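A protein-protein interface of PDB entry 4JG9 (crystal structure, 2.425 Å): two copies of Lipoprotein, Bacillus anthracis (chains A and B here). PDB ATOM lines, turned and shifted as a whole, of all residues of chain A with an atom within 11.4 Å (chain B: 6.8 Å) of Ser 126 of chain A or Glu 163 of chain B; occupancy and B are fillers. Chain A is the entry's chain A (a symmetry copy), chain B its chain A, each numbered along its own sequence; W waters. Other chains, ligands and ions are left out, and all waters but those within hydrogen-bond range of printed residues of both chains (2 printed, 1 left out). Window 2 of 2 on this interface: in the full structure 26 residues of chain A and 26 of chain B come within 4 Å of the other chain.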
ATOM      1  N   LYS A  87       3.026  -2.294   0.984  1.00  0.00           N
ATOM      2  CA  LYS A  87       2.242  -1.228   0.376  1.00  0.00           C
ATOM      3  C   LYS A  87       1.689  -1.724  -0.962  1.00  0.00           C
ATOM      4  O   LYS A  87       2.429  -2.218  -1.809  1.00  0.00           O
ATOM      5  CB  LYS A  87       3.092   0.039   0.195  1.00  0.00           C
ATOM      6  CG  LYS A  87       3.303   0.855   1.481  1.00  0.00           C
ATOM      7  CD  LYS A  87       4.781   1.216   1.714  1.00  0.00           C
ATOM      8  CE  LYS A  87       5.015   1.990   3.043  1.00  0.00           C
ATOM      9  NZ  LYS A  87       4.910   1.158   4.295  1.00  0.00           N
ATOM     10  N   THR A 117      -6.391   2.602  13.545  1.00  0.00           N
ATOM     11  CA  THR A 117      -5.178   2.977  12.861  1.00  0.00           C
ATOM     12  C   THR A 117      -5.507   3.424  11.459  1.00  0.00           C
ATOM     13  O   THR A 117      -6.505   3.014  10.889  1.00  0.00           O
ATOM     14  CB  THR A 117      -4.176   1.810  12.810  1.00  0.00           C
ATOM     15  OG1 THR A 117      -2.923   2.270  12.302  1.00  0.00           O
ATOM     16  CG2 THR A 117      -4.691   0.707  11.930  1.00  0.00           C
ATOM     17  N   PRO A 118      -4.672   4.291  10.918  1.00  0.00           N
ATOM     18  CA  PRO A 118      -4.804   4.717   9.533  1.00  0.00           C
ATOM     19  C   PRO A 118      -4.086   3.732   8.641  1.00  0.00           C
ATOM     20  O   PRO A 118      -3.124   3.122   9.080  1.00  0.00           O
ATOM     21  CB  PRO A 118      -4.083   6.060   9.516  1.00  0.00           C
ATOM     22  CG  PRO A 118      -3.104   5.972  10.621  1.00  0.00           C
ATOM     23  CD  PRO A 118      -3.790   5.179  11.684  1.00  0.00           C
ATOM     24  N   LEU A 119      -4.533   3.567   7.409  1.00  0.00           N
ATOM     25  CA  LEU A 119      -3.796   2.763   6.512  1.00  0.00           C
ATOM     26  C   LEU A 119      -3.397   3.514   5.273  1.00  0.00           C
ATOM     27  O   LEU A 119      -2.859   2.877   4.391  1.00  0.00           O
ATOM     28  CB  LEU A 119      -4.535   1.466   6.174  1.00  0.00           C
ATOM     29  CG  LEU A 119      -6.032   1.496   5.909  1.00  0.00           C
ATOM     30  CD1 LEU A 119      -6.353   2.281   4.652  1.00  0.00           C
ATOM     31  CD2 LEU A 119      -6.546   0.079   5.787  1.00  0.00           C
ATOM     32  N   LEU A 120      -3.612   4.796   5.116  1.00  0.00           N
ATOM     33  CA  LEU A 120      -3.165   5.342   3.846  1.00  0.00           C
ATOM     34  C   LEU A 120      -1.683   5.724   3.827  1.00  0.00           C
ATOM     35  O   LEU A 120      -1.190   6.373   4.731  1.00  0.00           O
ATOM     36  CB  LEU A 120      -4.062   6.483   3.387  1.00  0.00           C
ATOM     37  CG  LEU A 120      -5.484   6.077   3.034  1.00  0.00           C
ATOM     38  CD1 LEU A 120      -6.365   7.303   2.914  1.00  0.00           C
ATOM     39  CD2 LEU A 120      -5.511   5.264   1.757  1.00  0.00           C
ATOM     40  N   PHE A 121      -0.987   5.299   2.780  1.00  0.00           N
ATOM     41  CA  PHE A 121       0.404   5.655   2.548  1.00  0.00           C
ATOM     42  C   PHE A 121       0.438   6.202   1.143  1.00  0.00           C
ATOM     43  O   PHE A 121       0.755   5.504   0.198  1.00  0.00           O
ATOM     44  CB  PHE A 121       1.323   4.448   2.663  1.00  0.00           C
ATOM     45  CG  PHE A 121       1.646   4.064   4.072  1.00  0.00           C
ATOM     46  CD1 PHE A 121       0.950   3.059   4.702  1.00  0.00           C
ATOM     47  CD2 PHE A 121       2.643   4.710   4.764  1.00  0.00           C
ATOM     48  CE1 PHE A 121       1.244   2.702   5.996  1.00  0.00           C
ATOM     49  CE2 PHE A 121       2.947   4.359   6.059  1.00  0.00           C
ATOM     50  CZ  PHE A 121       2.245   3.352   6.677  1.00  0.00           C
ATOM     51  N   GLN A 122       0.081   7.467   1.019  1.00  0.00           N
ATOM     52  CA  GLN A 122      -0.124   8.092  -0.269  1.00  0.00           C
ATOM     53  C   GLN A 122       1.161   8.685  -0.858  1.00  0.00           C
ATOM     54  O   GLN A 122       1.930   9.362  -0.170  1.00  0.00           O
ATOM     55  CB  GLN A 122      -1.188   9.188  -0.131  1.00  0.00           C
ATOM     56  CG  GLN A 122      -2.600   8.659   0.119  1.00  0.00           C
ATOM     57  CD  GLN A 122      -3.137   7.813  -1.060  1.00  0.00           C
ATOM     58  OE1 GLN A 122      -2.753   6.654  -1.236  1.00  0.00           O
ATOM     59  NE2 GLN A 122      -4.029   8.400  -1.863  1.00  0.00           N
ATOM     60  N   GLN A 123       1.376   8.409  -2.138  1.00  0.00           N
ATOM     61  CA  GLN A 123       2.404   9.059  -2.938  1.00  0.00           C
ATOM     62  C   GLN A 123       3.792   8.945  -2.293  1.00  0.00           C
ATOM     63  O   GLN A 123       4.510   9.943  -2.140  1.00  0.00           O
ATOM     64  CB  GLN A 123       2.014  10.518  -3.184  1.00  0.00           C
ATOM     65  CG  GLN A 123       2.817  11.226  -4.279  1.00  0.00           C
ATOM     66  CD  GLN A 123       2.418  12.686  -4.434  1.00  0.00           C
ATOM     67  OE1 GLN A 123       1.475  13.003  -5.174  1.00  0.00           O
ATOM     68  NE2 GLN A 123       3.130  13.588  -3.725  1.00  0.00           N
ATOM     69  N   GLU A 124       4.137   7.720  -1.891  1.00  0.00           N
ATOM     70  CA  GLU A 124       5.442   7.413  -1.311  1.00  0.00           C
ATOM     71  C   GLU A 124       5.643   8.082   0.043  1.00  0.00           C
ATOM     72  O   GLU A 124       6.772   8.231   0.495  1.00  0.00           O
ATOM     73  CB  GLU A 124       6.583   7.786  -2.264  1.00  0.00           C
ATOM     74  CG  GLU A 124       6.541   7.052  -3.589  1.00  0.00           C
ATOM     75  CD  GLU A 124       6.799   5.562  -3.428  1.00  0.00           C
ATOM     76  OE1 GLU A 124       7.733   5.190  -2.679  1.00  0.00           O
ATOM     77  OE2 GLU A 124       6.062   4.763  -4.044  1.00  0.00           O
ATOM     78  N   SER A 125       4.556   8.493   0.690  1.00  0.00           N
ATOM     79  CA  SER A 125       4.676   9.083   2.016  1.00  0.00           C
ATOM     80  C   SER A 125       5.232   8.092   3.022  1.00  0.00           C
ATOM     81  O   SER A 125       4.984   6.883   2.936  1.00  0.00           O
ATOM     82  CB  SER A 125       3.320   9.540   2.527  1.00  0.00           C
ATOM     83  OG  SER A 125       3.432   9.929   3.882  1.00  0.00           O
ATOM     84  N   SER A 126       5.977   8.605   3.992  1.00  0.00           N
ATOM     85  CA  SER A 126       6.512   7.738   5.033  1.00  0.00           C
ATOM     86  C   SER A 126       5.491   7.620   6.173  1.00  0.00           C
ATOM     87  O   SER A 126       5.643   6.791   7.073  1.00  0.00           O
ATOM     88  CB  SER A 126       7.834   8.281   5.548  1.00  0.00           C
ATOM     89  OG  SER A 126       7.616   9.568   6.082  1.00  0.00           O
ATOM     90  N   GLU A 127       4.466   8.472   6.135  1.00  0.00           N
ATOM     91  CA  GLU A 127       3.454   8.518   7.184  1.00  0.00           C
ATOM     92  C   GLU A 127       2.093   7.979   6.755  1.00  0.00           C
ATOM     93  O   GLU A 127       1.586   8.308   5.685  1.00  0.00           O
ATOM     94  CB  GLU A 127       3.271   9.951   7.692  1.00  0.00           C
ATOM     95  CG  GLU A 127       4.516  10.548   8.391  1.00  0.00           C
ATOM     96  CD  GLU A 127       4.407  12.053   8.596  1.00  0.00           C
ATOM     97  OE1 GLU A 127       3.262  12.561   8.645  1.00  0.00           O
ATOM     98  OE2 GLU A 127       5.456  12.725   8.735  1.00  0.00           O
ATOM     99  N   PRO A 128       1.476   7.173   7.615  1.00  0.00           N
ATOM    100  CA  PRO A 128       0.115   6.704   7.371  1.00  0.00           C
ATOM    101  C   PRO A 128      -0.906   7.808   7.665  1.00  0.00           C
ATOM    102  O   PRO A 128      -0.819   8.477   8.708  1.00  0.00           O
ATOM    103  CB  PRO A 128      -0.036   5.554   8.367  1.00  0.00           C
ATOM    104  CG  PRO A 128       0.921   5.864   9.462  1.00  0.00           C
ATOM    105  CD  PRO A 128       2.051   6.636   8.859  1.00  0.00           C
ATOM    106  N   THR A 129      -1.851   8.013   6.749  1.00  0.00           N
ATOM    107  CA  THR A 129      -2.851   9.075   6.914  1.00  0.00           C
ATOM    108  C   THR A 129      -4.269   8.511   6.976  1.00  0.00           C
ATOM    109  O   THR A 129      -4.565   7.479   6.368  1.00  0.00           O
ATOM    110  CB  THR A 129      -2.768  10.106   5.782  1.00  0.00           C
ATOM    111  OG1 THR A 129      -2.735   9.419   4.519  1.00  0.00           O
ATOM    112  CG2 THR A 129      -1.493  10.943   5.929  1.00  0.00           C
ATOM    113  N   TRP A 130      -5.138   9.204   7.706  1.00  0.00           N
ATOM    114  CA  TRP A 130      -6.526   8.798   7.895  1.00  0.00           C
ATOM    115  C   TRP A 130      -7.327   9.084   6.643  1.00  0.00           C
ATOM    116  O   TRP A 130      -8.264   8.345   6.300  1.00  0.00           O
ATOM    117  CB  TRP A 130      -7.185   9.585   9.037  1.00  0.00           C
ATOM    118  CG  TRP A 130      -6.452   9.581  10.353  1.00  0.00           C
ATOM    119  CD1 TRP A 130      -5.646  10.571  10.846  1.00  0.00           C
ATOM    120  CD2 TRP A 130      -6.489   8.558  11.356  1.00  0.00           C
ATOM    121  NE1 TRP A 130      -5.177  10.220  12.098  1.00  0.00           N
ATOM    122  CE2 TRP A 130      -5.672   8.985  12.426  1.00  0.00           C
ATOM    123  CE3 TRP A 130      -7.137   7.320  11.454  1.00  0.00           C
ATOM    124  CZ2 TRP A 130      -5.479   8.219  13.581  1.00  0.00           C
ATOM    125  CZ3 TRP A 130      -6.934   6.552  12.604  1.00  0.00           C
ATOM    126  CH2 TRP A 130      -6.111   7.012  13.651  1.00  0.00           C
ATOM    127  N   THR A 146      -3.094   3.676  -1.997  1.00  0.00           N
ATOM    128  CA  THR A 146      -2.033   2.790  -1.550  1.00  0.00           C
ATOM    129  C   THR A 146      -2.209   2.508  -0.062  1.00  0.00           C
ATOM    130  O   THR A 146      -2.244   3.433   0.768  1.00  0.00           O
ATOM    131  CB  THR A 146      -0.645   3.379  -1.843  1.00  0.00           C
ATOM    132  OG1 THR A 146      -0.529   3.621  -3.251  1.00  0.00           O
ATOM    133  CG2 THR A 146       0.454   2.419  -1.425  1.00  0.00           C
ATOM    134  N   MET A 147      -2.326   1.227   0.270  1.00  0.00           N
ATOM    135  CA  MET A 147      -2.637   0.829   1.637  1.00  0.00           C
ATOM    136  C   MET A 147      -1.618  -0.133   2.192  1.00  0.00           C
ATOM    137  O   MET A 147      -0.915  -0.808   1.440  1.00  0.00           O
ATOM    138  CB  MET A 147      -4.003   0.148   1.686  1.00  0.00           C
ATOM    139  CG  MET A 147      -5.121   0.933   1.040  1.00  0.00           C
ATOM    140  SD  MET A 147      -6.868   0.067   1.250  1.00  0.00           S
ATOM    141  CE  MET A 147      -6.639  -1.335   0.045  1.00  0.00           C
ATOM    142  N   SER A 148      -1.575  -0.225   3.518  1.00  0.00           N
ATOM    143  CA  SER A 148      -0.754  -1.212   4.192  1.00  0.00           C
ATOM    144  C   SER A 148      -1.365  -1.539   5.555  1.00  0.00           C
ATOM    145  O   SER A 148      -1.770  -0.632   6.276  1.00  0.00           O
ATOM    146  CB  SER A 148       0.678  -0.690   4.349  1.00  0.00           C
ATOM    147  OG  SER A 148       1.542  -1.715   4.823  1.00  0.00           O
ATOM    148  N   ALA B  41       2.675   3.031  11.766  1.00  0.00           N
ATOM    149  CA  ALA B  41       3.473   4.129  12.271  1.00  0.00           C
ATOM    150  C   ALA B  41       4.293   4.659  11.099  1.00  0.00           C
ATOM    151  O   ALA B  41       4.413   3.992  10.074  1.00  0.00           O
ATOM    152  CB  ALA B  41       4.378   3.646  13.392  1.00  0.00           C
ATOM    153  N   PRO B  42       4.842   5.871  11.231  1.00  0.00           N
ATOM    154  CA  PRO B  42       5.710   6.366  10.157  1.00  0.00           C
ATOM    155  C   PRO B  42       6.915   5.448   9.973  1.00  0.00           C
ATOM    156  O   PRO B  42       7.376   4.838  10.933  1.00  0.00           O
ATOM    157  CB  PRO B  42       6.155   7.743  10.676  1.00  0.00           C
ATOM    158  CG  PRO B  42       5.036   8.168  11.591  1.00  0.00           C
ATOM    159  CD  PRO B  42       4.568   6.894  12.254  1.00  0.00           C
ATOM    160  N   SER B  43       7.425   5.351   8.751  1.00  0.00           N
ATOM    161  CA  SER B  43       8.541   4.444   8.490  1.00  0.00           C
ATOM    162  C   SER B  43       9.824   4.831   9.222  1.00  0.00           C
ATOM    163  O   SER B  43      10.714   4.000   9.376  1.00  0.00           O
ATOM    164  CB  SER B  43       8.816   4.355   6.999  1.00  0.00           C
ATOM    165  OG  SER B  43       9.331   5.586   6.537  1.00  0.00           O
ATOM    166  N   PHE B  44       9.934   6.088   9.646  1.00  0.00           N
ATOM    167  CA  PHE B  44      11.132   6.535  10.365  1.00  0.00           C
ATOM    168  C   PHE B  44      11.045   6.249  11.850  1.00  0.00           C
ATOM    169  O   PHE B  44      11.987   6.521  12.593  1.00  0.00           O
ATOM    170  CB  PHE B  44      11.467   8.016  10.100  1.00  0.00           C
ATOM    171  CG  PHE B  44      10.316   8.962  10.327  1.00  0.00           C
ATOM    172  CD1 PHE B  44      10.063   9.487  11.592  1.00  0.00           C
ATOM    173  CD2 PHE B  44       9.489   9.337   9.267  1.00  0.00           C
ATOM    174  CE1 PHE B  44       8.995  10.384  11.806  1.00  0.00           C
ATOM    175  CE2 PHE B  44       8.429  10.223   9.462  1.00  0.00           C
ATOM    176  CZ  PHE B  44       8.181  10.754  10.736  1.00  0.00           C
ATOM    177  N   PHE B  45       9.950   5.652  12.288  1.00  0.00           N
ATOM    178  CA  PHE B  45       9.832   5.305  13.687  1.00  0.00           C
ATOM    179  C   PHE B  45      10.214   3.861  13.938  1.00  0.00           C
ATOM    180  O   PHE B  45       9.718   2.956  13.286  1.00  0.00           O
ATOM    181  CB  PHE B  45       8.422   5.529  14.210  1.00  0.00           C
ATOM    182  CG  PHE B  45       8.193   4.922  15.559  1.00  0.00           C
ATOM    183  CD1 PHE B  45       8.616   5.567  16.698  1.00  0.00           C
ATOM    184  CD2 PHE B  45       7.582   3.695  15.684  1.00  0.00           C
ATOM    185  CE1 PHE B  45       8.420   5.008  17.940  1.00  0.00           C
ATOM    186  CE2 PHE B  45       7.384   3.128  16.922  1.00  0.00           C
ATOM    187  CZ  PHE B  45       7.802   3.788  18.052  1.00  0.00           C
ATOM    188  N   GLY B 102      13.471  21.461   9.032  1.00  0.00           N
ATOM    189  CA  GLY B 102      12.525  20.461   8.552  1.00  0.00           C
ATOM    190  C   GLY B 102      11.172  20.495   9.243  1.00  0.00           C
ATOM    191  O   GLY B 102      10.977  21.232  10.208  1.00  0.00           O
ATOM    192  N   LYS B 103      10.227  19.691   8.768  1.00  0.00           N
ATOM    193  CA  LYS B 103       8.964  19.593   9.480  1.00  0.00           C
ATOM    194  C   LYS B 103       9.235  18.870  10.801  1.00  0.00           C
ATOM    195  O   LYS B 103      10.114  18.001  10.886  1.00  0.00           O
ATOM    196  CB  LYS B 103       7.924  18.791   8.687  1.00  0.00           C
ATOM    197  CG  LYS B 103       7.717  19.204   7.259  1.00  0.00           C
ATOM    198  CD  LYS B 103       7.088  20.558   7.108  1.00  0.00           C
ATOM    199  CE  LYS B 103       6.658  20.722   5.647  1.00  0.00           C
ATOM    200  NZ  LYS B 103       6.564  22.154   5.284  1.00  0.00           N
ATOM    201  N   SER B 105       8.145  16.337  13.776  1.00  0.00           N
ATOM    202  CA  SER B 105       7.269  15.216  14.115  1.00  0.00           C
ATOM    203  C   SER B 105       7.368  14.834  15.589  1.00  0.00           C
ATOM    204  O   SER B 105       8.446  14.858  16.195  1.00  0.00           O
ATOM    205  CB  SER B 105       7.580  13.978  13.258  1.00  0.00           C
ATOM    206  OG  SER B 105       7.567  14.259  11.870  1.00  0.00           O
ATOM    207  N   THR B 131       2.980  15.155  12.341  1.00  0.00           N
ATOM    208  CA  THR B 131       3.954  16.135  11.884  1.00  0.00           C
ATOM    209  C   THR B 131       3.362  17.522  11.664  1.00  0.00           C
ATOM    210  O   THR B 131       2.256  17.654  11.146  1.00  0.00           O
ATOM    211  CB  THR B 131       4.569  15.625  10.559  1.00  0.00           C
ATOM    212  OG1 THR B 131       5.150  14.333  10.779  1.00  0.00           O
ATOM    213  CG2 THR B 131       5.622  16.587   9.998  1.00  0.00           C
ATOM    214  N   TYR B 160      11.294  14.164  15.990  1.00  0.00           N
ATOM    215  CA  TYR B 160      12.014  14.036  14.728  1.00  0.00           C
ATOM    216  C   TYR B 160      11.957  15.369  14.015  1.00  0.00           C
ATOM    217  O   TYR B 160      11.001  16.126  14.168  1.00  0.00           O
ATOM    218  CB  TYR B 160      11.384  12.944  13.844  1.00  0.00           C
ATOM    219  CG  TYR B 160      11.339  11.594  14.519  1.00  0.00           C
ATOM    220  CD1 TYR B 160      12.223  10.581  14.156  1.00  0.00           C
ATOM    221  CD2 TYR B 160      10.411  11.333  15.530  1.00  0.00           C
ATOM    222  CE1 TYR B 160      12.193   9.341  14.789  1.00  0.00           C
ATOM    223  CE2 TYR B 160      10.378  10.096  16.174  1.00  0.00           C
ATOM    224  CZ  TYR B 160      11.267   9.110  15.796  1.00  0.00           C
ATOM    225  OH  TYR B 160      11.220   7.893  16.432  1.00  0.00           O
ATOM    226  N   VAL B 161      13.010  15.675  13.275  1.00  0.00           N
ATOM    227  CA  VAL B 161      13.007  16.817  12.390  1.00  0.00           C
ATOM    228  C   VAL B 161      13.454  16.337  11.036  1.00  0.00           C
ATOM    229  O   VAL B 161      14.491  15.652  10.918  1.00  0.00           O
ATOM    230  CB  VAL B 161      13.939  17.939  12.886  1.00  0.00           C
ATOM    231  CG1 VAL B 161      14.077  19.039  11.829  1.00  0.00           C
ATOM    232  CG2 VAL B 161      13.440  18.476  14.214  1.00  0.00           C
ATOM    233  N   ASN B 162      12.663  16.681  10.025  1.00  0.00           N
ATOM    234  CA  ASN B 162      12.940  16.236   8.669  1.00  0.00           C
ATOM    235  C   ASN B 162      13.075  14.716   8.639  1.00  0.00           C
ATOM    236  O   ASN B 162      13.909  14.176   7.909  1.00  0.00           O
ATOM    237  CB  ASN B 162      14.197  16.911   8.116  1.00  0.00           C
ATOM    238  CG  ASN B 162      14.223  16.921   6.603  1.00  0.00           C
ATOM    239  OD1 ASN B 162      13.173  16.832   5.958  1.00  0.00           O
ATOM    240  ND2 ASN B 162      15.417  17.035   6.023  1.00  0.00           N
ATOM    241  N   GLU B 163      12.264  14.052   9.471  1.00  0.00           N
ATOM    242  CA  GLU B 163      12.192  12.585   9.550  1.00  0.00           C
ATOM    243  C   GLU B 163      13.396  11.912  10.175  1.00  0.00           C
ATOM    244  O   GLU B 163      13.496  10.686  10.151  1.00  0.00           O
ATOM    245  CB  GLU B 163      11.886  11.961   8.175  1.00  0.00           C
ATOM    246  CG  GLU B 163      10.600  12.481   7.588  1.00  0.00           C
ATOM    247  CD  GLU B 163      10.050  11.606   6.474  1.00  0.00           C
ATOM    248  OE1 GLU B 163      10.744  10.637   6.080  1.00  0.00           O
ATOM    249  OE2 GLU B 163       8.910  11.888   6.012  1.00  0.00           O
ATOM    250  N   LYS B 164      14.299  12.717  10.728  1.00  0.00           N
ATOM    251  CA  LYS B 164      15.487  12.221  11.423  1.00  0.00           C
ATOM    252  C   LYS B 164      15.327  12.399  12.931  1.00  0.00           C
ATOM    253  O   LYS B 164      14.890  13.460  13.387  1.00  0.00           O
ATOM    254  CB  LYS B 164      16.721  12.971  10.931  1.00  0.00           C
ATOM    255  CG  LYS B 164      18.028  12.606  11.620  1.00  0.00           C
ATOM    256  CD  LYS B 164      19.146  13.474  11.063  1.00  0.00           C
ATOM    257  CE  LYS B 164      20.429  13.296  11.820  1.00  0.00           C
ATOM    258  NZ  LYS B 164      21.056  11.986  11.527  1.00  0.00           N
ATOM    259  N   TYR B 165      15.643  11.356  13.695  1.00  0.00           N
ATOM    260  CA  TYR B 165      15.503  11.403  15.150  1.00  0.00           C
ATOM    261  C   TYR B 165      16.283  12.568  15.759  1.00  0.00           C
ATOM    262  O   TYR B 165      17.452  12.779  15.441  1.00  0.00           O
ATOM    263  CB  TYR B 165      15.956  10.082  15.776  1.00  0.00           C
ATOM    264  CG  TYR B 165      15.848  10.055  17.280  1.00  0.00           C
ATOM    265  CD1 TYR B 165      14.647   9.735  17.906  1.00  0.00           C
ATOM    266  CD2 TYR B 165      16.945  10.347  18.082  1.00  0.00           C
ATOM    267  CE1 TYR B 165      14.543   9.713  19.292  1.00  0.00           C
ATOM    268  CE2 TYR B 165      16.849  10.324  19.469  1.00  0.00           C
ATOM    269  CZ  TYR B 165      15.648  10.012  20.065  1.00  0.00           C
ATOM    270  OH  TYR B 165      15.552   9.991  21.441  1.00  0.00           O
HETATM  271  O   HOH W   1       6.778  11.479   3.790  1.00  0.00           O
HETATM  272  O   HOH W   2       1.297  14.061   9.819  1.00  0.00           O
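The side-chain hydroxyl (OG) of Ser 126 of chain A lies within hydrogen-bond range of the side-chain carboxylate (OE2) of Glu 163 of chain B (2.7 Å).
The side-chain carboxylate (OE2) of Glu 127 of chain A lies within hydrogen-bond range of the side-chain hydroxyl (OG1) of Thr 131 of chain B (2.6 Å).
The backbone NH (N) of Ser 43 of chain B is in hydrogen-bond range of the backbone carbonyl oxygen (O) of Ser 126 of chain A.
The backbone NH of Glu 127 of chain A sits at hydrogen-bond distance from the side-chain hydroxyl of Ser 125 of chain A.
The side-chain hydroxyl (OG) of Ser 105 of chain B is in hydrogen-bond range of the side-chain hydroxyl (OG1) of Thr 131 of chain B, at 2.7 Å.
O of Ser 126 of chain A touches CA of Pro 42 of chain B, 3.1 Å away.
Ser 126 of chain A touches Phe 44 of chain B (OG to CE2, 3.5 Å).
Glu 127 of chain A touches Pro 42 of chain B.
Glu 127 of chain A touches Phe 44 of chain B (OE2 to CZ, 3.9 Å).
Pro 128 of chain A touches Ala 41 of chain B (CD to C, 3.7 Å).
Pro 128 of chain A touches Pro 42 of chain B (CD to N, 3.7 Å).
Of the printed residues of chain B, Glu 127 of chain A touches Pro 42, Phe 44 and Thr 131.
Of the printed residues of chain B, Pro 128 of chain A touches Ala 41 and Pro 42.
Pro 42 of chain B touches three residues of chain A.
Of chain A, only Ser 126 comes within 4 Å of Ser 43 of chain B.
Printed residues of chain A within 4 Å of Thr 131 of chain B: Glu 127 (2.6 Å).
Printed residues of chain A within 4 Å of Glu 163 of chain B: Ser 126 (2.7 Å).
Of the 15 printed residues of chain B, 6 touch a printed residue of chain A.
Among the printed residues, 9 pairs touch across the chains.
Among the printed residues, no Asp or Glu carboxylate lies within 4 Å of a Lys or Arg side-chain nitrogen of the other chain.
No position is printed for both chains.
Of the 9 pairs that touch across the chains among the printed residues, none has its exchanged pair printed and touching as well.
Water W2 lies within hydrogen-bond range of the side-chain carboxylate (OE1) of Glu 127 of chain A and the backbone NH (N) of Thr 131 of chain B.
Water W1 lies within hydrogen-bond range of the backbone NH (N) of Ser 126 of chain A and the side-chain carboxylate (OE2) of Glu 163 of chain B.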
